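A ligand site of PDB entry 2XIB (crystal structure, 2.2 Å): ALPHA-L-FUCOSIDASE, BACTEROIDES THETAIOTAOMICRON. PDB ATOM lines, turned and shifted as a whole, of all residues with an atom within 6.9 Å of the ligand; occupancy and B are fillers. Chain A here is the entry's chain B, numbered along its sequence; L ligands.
An oxygen (O2) of the ligand lies within hydrogen-bond range of the side-chain carboxylate of Glu 56 (2.6 Å).
The side-chain carboxylate (OD2) of Asp 198 lies within salt-bridge range of a nitrogen (N1) of the ligand, at 2.7 Å.
A ring nitrogen (NE2) of His 105 sits at hydrogen-bond distance from an oxygen (O3) of the ligand (2.7 Å).
A ring nitrogen (NE2) of His 104 lies within hydrogen-bond range of an oxygen (O1) of the ligand (2.8 Å).
A ring nitrogen (NE2) of His 35 is in hydrogen-bond range of an oxygen (O1) of the ligand (2.9 Å).
O3 of the ligand lies within hydrogen-bond range of NE1 of Trp 57.
A nitrogen (N1) of the ligand lies within salt-bridge range of the side-chain carboxylate of Glu 257 (3.1 Å).
OH of Tyr 147 sits at hydrogen-bond distance from O1 of the ligand (3.4 Å).
Residues that only touch the ligand: Trp 196, Trp 201, Arg 231 and Trp 285.
Hydrophobic or aromatic side chains that line the ligand: His 35, Trp 57, His 104, His 105, Tyr 147, Trp 196, Trp 201 and Trp 285.
Within 4 Å of the ligand: His 35, Glu 56, Trp 57, His 104, His 105, Tyr 147, Trp 196, Asp 198, Trp 201, Arg 231, Glu 257 and Trp 285.
The nearest printed residue that does not touch the ligand is Cys 277 (4.6 Å).
The side-chain carboxylate (OE1) of Glu 56 is in hydrogen-bond range of the backbone NH (N) of Trp 285.
The backbone NH (N) of Gly 286 is in hydrogen-bond range of the side-chain carboxylate (OE1) of Glu 56 (3.1 Å).
OD2 of Asp 198 is in hydrogen-bond range of OH of Tyr 147 (2.6 Å).
The guanidinium group (NH1) of Arg 231 lies within salt-bridge range of the side-chain carboxylate (OD1) of Asp 198 (2.9 Å).
A ring nitrogen (NE2) of His 104 sits close to the side-chain hydroxyl (OH) of Tyr 147, at 3.2 Å.
A ring nitrogen (ND1) of His 35 lies within hydrogen-bond range of the side-chain amide oxygen (OD1) of Asn 319 (2.7 Å).
NH2 of Arg 231 lies within salt-bridge range of OE1 of Glu 257 (3.0 Å).
O of Trp 285 is in hydrogen-bond range of ND2 of Asn 319.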
ATOM      1  N   PHE A  33      -8.374  -1.200 -10.983  1.00  0.00           N
ATOM      2  CA  PHE A  33      -9.494  -2.068 -10.595  1.00  0.00           C
ATOM      3  C   PHE A  33      -9.712  -1.873  -9.083  1.00  0.00           C
ATOM      4  O   PHE A  33      -8.745  -1.766  -8.344  1.00  0.00           O
ATOM      5  CB  PHE A  33      -9.175  -3.551 -10.842  1.00  0.00           C
ATOM      6  CG  PHE A  33     -10.231  -4.294 -11.616  1.00  0.00           C
ATOM      7  CD1 PHE A  33      -9.881  -5.041 -12.742  1.00  0.00           C
ATOM      8  CD2 PHE A  33     -11.551  -4.235 -11.251  1.00  0.00           C
ATOM      9  CE1 PHE A  33     -10.828  -5.721 -13.470  1.00  0.00           C
ATOM     10  CE2 PHE A  33     -12.526  -4.913 -11.963  1.00  0.00           C
ATOM     11  CZ  PHE A  33     -12.152  -5.659 -13.092  1.00  0.00           C
ATOM     12  N   HIS A  35     -11.657  -4.006  -6.211  1.00  0.00           N
ATOM     13  CA  HIS A  35     -12.410  -5.153  -5.705  1.00  0.00           C
ATOM     14  C   HIS A  35     -12.675  -4.868  -4.222  1.00  0.00           C
ATOM     15  O   HIS A  35     -11.800  -5.043  -3.375  1.00  0.00           O
ATOM     16  CB  HIS A  35     -11.602  -6.447  -5.815  1.00  0.00           C
ATOM     17  CG  HIS A  35     -11.679  -7.095  -7.159  1.00  0.00           C
ATOM     18  ND1 HIS A  35     -11.020  -6.584  -8.257  1.00  0.00           N
ATOM     19  CD2 HIS A  35     -12.338  -8.196  -7.583  1.00  0.00           C
ATOM     20  CE1 HIS A  35     -11.273  -7.348  -9.302  1.00  0.00           C
ATOM     21  NE2 HIS A  35     -12.067  -8.328  -8.927  1.00  0.00           N
ATOM     22  N   ALA A  54      -7.354 -16.845  -3.177  1.00  0.00           N
ATOM     23  CA  ALA A  54      -7.823 -15.464  -3.343  1.00  0.00           C
ATOM     24  C   ALA A  54      -8.876 -15.117  -2.302  1.00  0.00           C
ATOM     25  O   ALA A  54      -9.858 -15.865  -2.087  1.00  0.00           O
ATOM     26  CB  ALA A  54      -8.363 -15.248  -4.739  1.00  0.00           C
ATOM     27  N   GLU A  56     -11.261 -12.885  -2.060  1.00  0.00           N
ATOM     28  CA  GLU A  56     -12.650 -12.725  -2.499  1.00  0.00           C
ATOM     29  C   GLU A  56     -13.402 -14.066  -2.699  1.00  0.00           C
ATOM     30  O   GLU A  56     -14.656 -14.075  -2.750  1.00  0.00           O
ATOM     31  CB  GLU A  56     -12.772 -11.791  -3.708  1.00  0.00           C
ATOM     32  CG  GLU A  56     -12.393 -12.325  -5.104  1.00  0.00           C
ATOM     33  CD  GLU A  56     -10.913 -12.604  -5.304  1.00  0.00           C
ATOM     34  OE1 GLU A  56     -10.090 -12.250  -4.418  1.00  0.00           O
ATOM     35  OE2 GLU A  56     -10.579 -13.202  -6.369  1.00  0.00           O
ATOM     36  N   TRP A  57     -12.658 -15.159  -2.811  1.00  0.00           N
ATOM     37  CA  TRP A  57     -13.212 -16.529  -2.858  1.00  0.00           C
ATOM     38  C   TRP A  57     -13.223 -17.274  -1.499  1.00  0.00           C
ATOM     39  O   TRP A  57     -13.325 -18.483  -1.470  1.00  0.00           O
ATOM     40  CB  TRP A  57     -12.424 -17.390  -3.888  1.00  0.00           C
ATOM     41  CG  TRP A  57     -12.807 -17.155  -5.313  1.00  0.00           C
ATOM     42  CD1 TRP A  57     -12.438 -16.101  -6.102  1.00  0.00           C
ATOM     43  CD2 TRP A  57     -13.642 -17.984  -6.132  1.00  0.00           C
ATOM     44  NE1 TRP A  57     -13.013 -16.217  -7.355  1.00  0.00           N
ATOM     45  CE2 TRP A  57     -13.737 -17.377  -7.403  1.00  0.00           C
ATOM     46  CE3 TRP A  57     -14.322 -19.189  -5.908  1.00  0.00           C
ATOM     47  CZ2 TRP A  57     -14.485 -17.931  -8.441  1.00  0.00           C
ATOM     48  CZ3 TRP A  57     -15.052 -19.748  -6.934  1.00  0.00           C
ATOM     49  CH2 TRP A  57     -15.146 -19.116  -8.182  1.00  0.00           C
ATOM     50  N   THR A 101     -16.089  -3.219  -8.716  1.00  0.00           N
ATOM     51  CA  THR A 101     -16.955  -4.328  -8.375  1.00  0.00           C
ATOM     52  C   THR A 101     -18.260  -3.763  -7.769  1.00  0.00           C
ATOM     53  O   THR A 101     -18.301  -3.388  -6.566  1.00  0.00           O
ATOM     54  CB  THR A 101     -16.272  -5.249  -7.361  1.00  0.00           C
ATOM     55  OG1 THR A 101     -15.942  -4.491  -6.175  1.00  0.00           O
ATOM     56  CG2 THR A 101     -14.985  -5.870  -7.948  1.00  0.00           C
ATOM     57  N   HIS A 104     -19.702  -8.541  -6.460  1.00  0.00           N
ATOM     58  CA  HIS A 104     -18.781  -9.641  -6.761  1.00  0.00           C
ATOM     59  C   HIS A 104     -19.541 -10.973  -6.568  1.00  0.00           C
ATOM     60  O   HIS A 104     -20.767 -10.955  -6.462  1.00  0.00           O
ATOM     61  CB  HIS A 104     -17.473  -9.539  -6.016  1.00  0.00           C
ATOM     62  CG  HIS A 104     -16.374 -10.352  -6.633  1.00  0.00           C
ATOM     63  ND1 HIS A 104     -16.134 -11.660  -6.270  1.00  0.00           N
ATOM     64  CD2 HIS A 104     -15.488 -10.075  -7.613  1.00  0.00           C
ATOM     65  CE1 HIS A 104     -15.145 -12.143  -6.996  1.00  0.00           C
ATOM     66  NE2 HIS A 104     -14.726 -11.190  -7.805  1.00  0.00           N
ATOM     67  N   HIS A 105     -18.874 -12.125  -6.629  1.00  0.00           N
ATOM     68  CA  HIS A 105     -19.596 -13.414  -6.603  1.00  0.00           C
ATOM     69  C   HIS A 105     -20.468 -13.550  -5.350  1.00  0.00           C
ATOM     70  O   HIS A 105     -21.535 -14.137  -5.402  1.00  0.00           O
ATOM     71  CB  HIS A 105     -18.672 -14.648  -6.671  1.00  0.00           C
ATOM     72  CG  HIS A 105     -17.670 -14.616  -7.783  1.00  0.00           C
ATOM     73  ND1 HIS A 105     -17.969 -14.181  -9.063  1.00  0.00           N
ATOM     74  CD2 HIS A 105     -16.365 -15.003  -7.821  1.00  0.00           C
ATOM     75  CE1 HIS A 105     -16.897 -14.300  -9.831  1.00  0.00           C
ATOM     76  NE2 HIS A 105     -15.912 -14.793  -9.103  1.00  0.00           N
ATOM     77  N   TYR A 147     -17.804  -3.367 -12.988  1.00  0.00           N
ATOM     78  CA  TYR A 147     -17.656  -4.810 -12.911  1.00  0.00           C
ATOM     79  C   TYR A 147     -18.991  -5.355 -12.414  1.00  0.00           C
ATOM     80  O   TYR A 147     -19.593  -4.780 -11.532  1.00  0.00           O
ATOM     81  CB  TYR A 147     -16.510  -5.179 -11.924  1.00  0.00           C
ATOM     82  CG  TYR A 147     -16.427  -6.662 -11.551  1.00  0.00           C
ATOM     83  CD1 TYR A 147     -15.312  -7.436 -11.911  1.00  0.00           C
ATOM     84  CD2 TYR A 147     -17.457  -7.288 -10.824  1.00  0.00           C
ATOM     85  CE1 TYR A 147     -15.245  -8.814 -11.593  1.00  0.00           C
ATOM     86  CE2 TYR A 147     -17.394  -8.662 -10.493  1.00  0.00           C
ATOM     87  CZ  TYR A 147     -16.288  -9.406 -10.893  1.00  0.00           C
ATOM     88  OH  TYR A 147     -16.221 -10.727 -10.561  1.00  0.00           O
ATOM     89  N   MET A 151     -22.689 -14.678 -11.885  1.00  0.00           N
ATOM     90  CA  MET A 151     -22.725 -15.685 -10.820  1.00  0.00           C
ATOM     91  C   MET A 151     -22.972 -14.992  -9.467  1.00  0.00           C
ATOM     92  O   MET A 151     -22.188 -14.142  -9.065  1.00  0.00           O
ATOM     93  CB  MET A 151     -21.404 -16.466 -10.769  1.00  0.00           C
ATOM     94  CG  MET A 151     -21.373 -17.581  -9.735  1.00  0.00           C
ATOM     95  SD  MET A 151     -19.845 -18.519  -9.668  1.00  0.00           S
ATOM     96  CE  MET A 151     -18.700 -17.202  -9.331  1.00  0.00           C
ATOM     97  N   TRP A 196     -18.242  -4.595 -17.265  1.00  0.00           N
ATOM     98  CA  TRP A 196     -17.301  -5.704 -17.326  1.00  0.00           C
ATOM     99  C   TRP A 196     -17.919  -6.874 -16.587  1.00  0.00           C
ATOM    100  O   TRP A 196     -17.919  -6.925 -15.355  1.00  0.00           O
ATOM    101  CB  TRP A 196     -15.984  -5.336 -16.666  1.00  0.00           C
ATOM    102  CG  TRP A 196     -14.833  -6.234 -17.030  1.00  0.00           C
ATOM    103  CD1 TRP A 196     -14.030  -6.109 -18.131  1.00  0.00           C
ATOM    104  CD2 TRP A 196     -14.340  -7.350 -16.307  1.00  0.00           C
ATOM    105  NE1 TRP A 196     -13.073  -7.072 -18.138  1.00  0.00           N
ATOM    106  CE2 TRP A 196     -13.222  -7.848 -17.013  1.00  0.00           C
ATOM    107  CE3 TRP A 196     -14.713  -7.978 -15.110  1.00  0.00           C
ATOM    108  CZ2 TRP A 196     -12.482  -8.962 -16.586  1.00  0.00           C
ATOM    109  CZ3 TRP A 196     -13.956  -9.098 -14.670  1.00  0.00           C
ATOM    110  CH2 TRP A 196     -12.866  -9.568 -15.405  1.00  0.00           C
ATOM    111  N   ASP A 198     -18.437 -10.755 -15.397  1.00  0.00           N
ATOM    112  CA  ASP A 198     -17.637 -11.842 -14.865  1.00  0.00           C
ATOM    113  C   ASP A 198     -18.568 -12.954 -14.374  1.00  0.00           C
ATOM    114  O   ASP A 198     -19.778 -12.765 -14.259  1.00  0.00           O
ATOM    115  CB  ASP A 198     -16.769 -11.318 -13.723  1.00  0.00           C
ATOM    116  CG  ASP A 198     -15.533 -12.162 -13.479  1.00  0.00           C
ATOM    117  OD1 ASP A 198     -15.160 -13.018 -14.314  1.00  0.00           O
ATOM    118  OD2 ASP A 198     -14.897 -11.956 -12.439  1.00  0.00           O
ATOM    119  N   GLY A 199     -17.996 -14.107 -14.051  1.00  0.00           N
ATOM    120  CA  GLY A 199     -18.734 -15.210 -13.448  1.00  0.00           C
ATOM    121  C   GLY A 199     -19.784 -15.728 -14.410  1.00  0.00           C
ATOM    122  O   GLY A 199     -20.905 -16.037 -14.010  1.00  0.00           O
ATOM    123  N   TRP A 201     -19.151 -18.318 -16.716  1.00  0.00           N
ATOM    124  CA  TRP A 201     -18.606 -19.560 -17.308  1.00  0.00           C
ATOM    125  C   TRP A 201     -19.399 -20.833 -16.980  1.00  0.00           C
ATOM    126  O   TRP A 201     -19.099 -21.896 -17.543  1.00  0.00           O
ATOM    127  CB  TRP A 201     -17.131 -19.773 -16.850  1.00  0.00           C
ATOM    128  CG  TRP A 201     -16.969 -19.637 -15.369  1.00  0.00           C
ATOM    129  CD1 TRP A 201     -17.387 -20.522 -14.420  1.00  0.00           C
ATOM    130  CD2 TRP A 201     -16.416 -18.522 -14.680  1.00  0.00           C
ATOM    131  NE1 TRP A 201     -17.120 -20.021 -13.164  1.00  0.00           N
ATOM    132  CE2 TRP A 201     -16.519 -18.800 -13.297  1.00  0.00           C
ATOM    133  CE3 TRP A 201     -15.824 -17.336 -15.084  1.00  0.00           C
ATOM    134  CZ2 TRP A 201     -16.050 -17.905 -12.320  1.00  0.00           C
ATOM    135  CZ3 TRP A 201     -15.355 -16.454 -14.118  1.00  0.00           C
ATOM    136  CH2 TRP A 201     -15.476 -16.740 -12.760  1.00  0.00           C
ATOM    137  N   ARG A 231     -16.308 -11.192 -22.189  1.00  0.00           N
ATOM    138  CA  ARG A 231     -16.563 -12.235 -21.211  1.00  0.00           C
ATOM    139  C   ARG A 231     -18.066 -12.496 -20.907  1.00  0.00           C
ATOM    140  O   ARG A 231     -18.429 -13.593 -20.466  1.00  0.00           O
ATOM    141  CB  ARG A 231     -15.787 -11.945 -19.936  1.00  0.00           C
ATOM    142  CG  ARG A 231     -15.793 -13.124 -18.975  1.00  0.00           C
ATOM    143  CD  ARG A 231     -15.032 -12.832 -17.726  1.00  0.00           C
ATOM    144  NE  ARG A 231     -13.629 -12.536 -17.996  1.00  0.00           N
ATOM    145  CZ  ARG A 231     -12.627 -12.858 -17.191  1.00  0.00           C
ATOM    146  NH1 ARG A 231     -12.834 -13.493 -16.029  1.00  0.00           N
ATOM    147  NH2 ARG A 231     -11.397 -12.520 -17.559  1.00  0.00           N
ATOM    148  N   GLU A 257      -6.201 -12.231 -18.049  1.00  0.00           N
ATOM    149  CA  GLU A 257      -6.326 -11.979 -16.621  1.00  0.00           C
ATOM    150  C   GLU A 257      -5.124 -12.629 -15.928  1.00  0.00           C
ATOM    151  O   GLU A 257      -4.967 -13.865 -15.950  1.00  0.00           O
ATOM    152  CB  GLU A 257      -7.660 -12.558 -16.137  1.00  0.00           C
ATOM    153  CG  GLU A 257      -7.896 -12.488 -14.633  1.00  0.00           C
ATOM    154  CD  GLU A 257      -9.295 -12.961 -14.245  1.00  0.00           C
ATOM    155  OE1 GLU A 257     -10.278 -12.387 -14.754  1.00  0.00           O
ATOM    156  OE2 GLU A 257      -9.399 -13.910 -13.438  1.00  0.00           O
ATOM    157  N   CYS A 277      -6.230  -7.293 -17.191  1.00  0.00           N
ATOM    158  CA  CYS A 277      -6.300  -6.916 -15.800  1.00  0.00           C
ATOM    159  C   CYS A 277      -5.272  -7.723 -15.029  1.00  0.00           C
ATOM    160  O   CYS A 277      -4.974  -8.859 -15.399  1.00  0.00           O
ATOM    161  CB  CYS A 277      -7.711  -7.125 -15.247  1.00  0.00           C
ATOM    162  SG  CYS A 277      -8.311  -8.772 -15.418  1.00  0.00           S
ATOM    163  N   THR A 279      -3.304  -8.447 -10.910  1.00  0.00           N
ATOM    164  CA  THR A 279      -3.154  -8.303  -9.478  1.00  0.00           C
ATOM    165  C   THR A 279      -1.709  -7.892  -9.139  1.00  0.00           C
ATOM    166  O   THR A 279      -0.788  -8.049  -9.962  1.00  0.00           O
ATOM    167  CB  THR A 279      -3.527  -9.618  -8.755  1.00  0.00           C
ATOM    168  OG1 THR A 279      -2.762 -10.700  -9.301  1.00  0.00           O
ATOM    169  CG2 THR A 279      -5.002  -9.919  -8.913  1.00  0.00           C
ATOM    170  N   ASN A 283      -2.231 -13.955  -6.915  1.00  0.00           N
ATOM    171  CA  ASN A 283      -3.656 -14.144  -7.131  1.00  0.00           C
ATOM    172  C   ASN A 283      -4.498 -13.676  -5.916  1.00  0.00           C
ATOM    173  O   ASN A 283      -5.103 -14.476  -5.215  1.00  0.00           O
ATOM    174  CB  ASN A 283      -3.973 -15.611  -7.427  1.00  0.00           C
ATOM    175  CG  ASN A 283      -5.373 -15.791  -8.022  1.00  0.00           C
ATOM    176  OD1 ASN A 283      -6.153 -14.840  -8.113  1.00  0.00           O
ATOM    177  ND2 ASN A 283      -5.686 -17.005  -8.425  1.00  0.00           N
ATOM    178  N   TRP A 285      -7.351 -10.489  -5.355  1.00  0.00           N
ATOM    179  CA  TRP A 285      -8.106  -9.372  -5.921  1.00  0.00           C
ATOM    180  C   TRP A 285      -8.753  -8.561  -4.799  1.00  0.00           C
ATOM    181  O   TRP A 285      -8.566  -7.359  -4.739  1.00  0.00           O
ATOM    182  CB  TRP A 285      -9.173  -9.869  -6.930  1.00  0.00           C
ATOM    183  CG  TRP A 285      -8.615 -10.565  -8.157  1.00  0.00           C
ATOM    184  CD1 TRP A 285      -8.446 -11.908  -8.328  1.00  0.00           C
ATOM    185  CD2 TRP A 285      -8.241  -9.955  -9.401  1.00  0.00           C
ATOM    186  NE1 TRP A 285      -7.963 -12.164  -9.588  1.00  0.00           N
ATOM    187  CE2 TRP A 285      -7.819 -10.989 -10.259  1.00  0.00           C
ATOM    188  CE3 TRP A 285      -8.195  -8.638  -9.865  1.00  0.00           C
ATOM    189  CZ2 TRP A 285      -7.364 -10.738 -11.552  1.00  0.00           C
ATOM    190  CZ3 TRP A 285      -7.758  -8.397 -11.136  1.00  0.00           C
ATOM    191  CH2 TRP A 285      -7.338  -9.436 -11.970  1.00  0.00           C
ATOM    192  N   GLY A 286      -9.510  -9.218  -3.940  1.00  0.00           N
ATOM    193  CA  GLY A 286      -9.978  -8.601  -2.708  1.00  0.00           C
ATOM    194  C   GLY A 286      -8.862  -8.448  -1.683  1.00  0.00           C
ATOM    195  O   GLY A 286      -7.793  -8.983  -1.849  1.00  0.00           O
ATOM    196  N   ASN A 319      -5.108  -3.712 -10.339  1.00  0.00           N
ATOM    197  CA  ASN A 319      -6.066  -3.956  -9.272  1.00  0.00           C
ATOM    198  C   ASN A 319      -5.591  -3.517  -7.905  1.00  0.00           C
ATOM    199  O   ASN A 319      -4.400  -3.628  -7.572  1.00  0.00           O
ATOM    200  CB  ASN A 319      -6.413  -5.418  -9.186  1.00  0.00           C
ATOM    201  CG  ASN A 319      -7.426  -5.706  -8.067  1.00  0.00           C
ATOM    202  OD1 ASN A 319      -8.603  -5.378  -8.193  1.00  0.00           O
ATOM    203  ND2 ASN A 319      -6.964  -6.306  -6.974  1.00  0.00           N
HETATM  204  C1  LIG L   1     -12.382 -13.697 -11.852  1.00  0.00           C
HETATM  205  C2  LIG L   1     -12.926 -13.672 -10.431  1.00  0.00           C
HETATM  206  C3  LIG L   1     -11.888 -13.084  -9.528  1.00  0.00           C
HETATM  207  C4  LIG L   1     -11.640 -11.659 -10.041  1.00  0.00           C
HETATM  208  C5  LIG L   1     -11.191 -11.667 -11.512  1.00  0.00           C
HETATM  209  C6  LIG L   1     -10.981 -10.251 -12.039  1.00  0.00           C
HETATM  210  O1  LIG L   1     -12.881 -10.902  -9.931  1.00  0.00           O
HETATM  211  O2  LIG L   1     -12.376 -13.048  -8.172  1.00  0.00           O
HETATM  212  O3  LIG L   1     -13.321 -14.981  -9.969  1.00  0.00           O
HETATM  213  N1  LIG L   1     -12.196 -12.308 -12.332  1.00  0.00           N
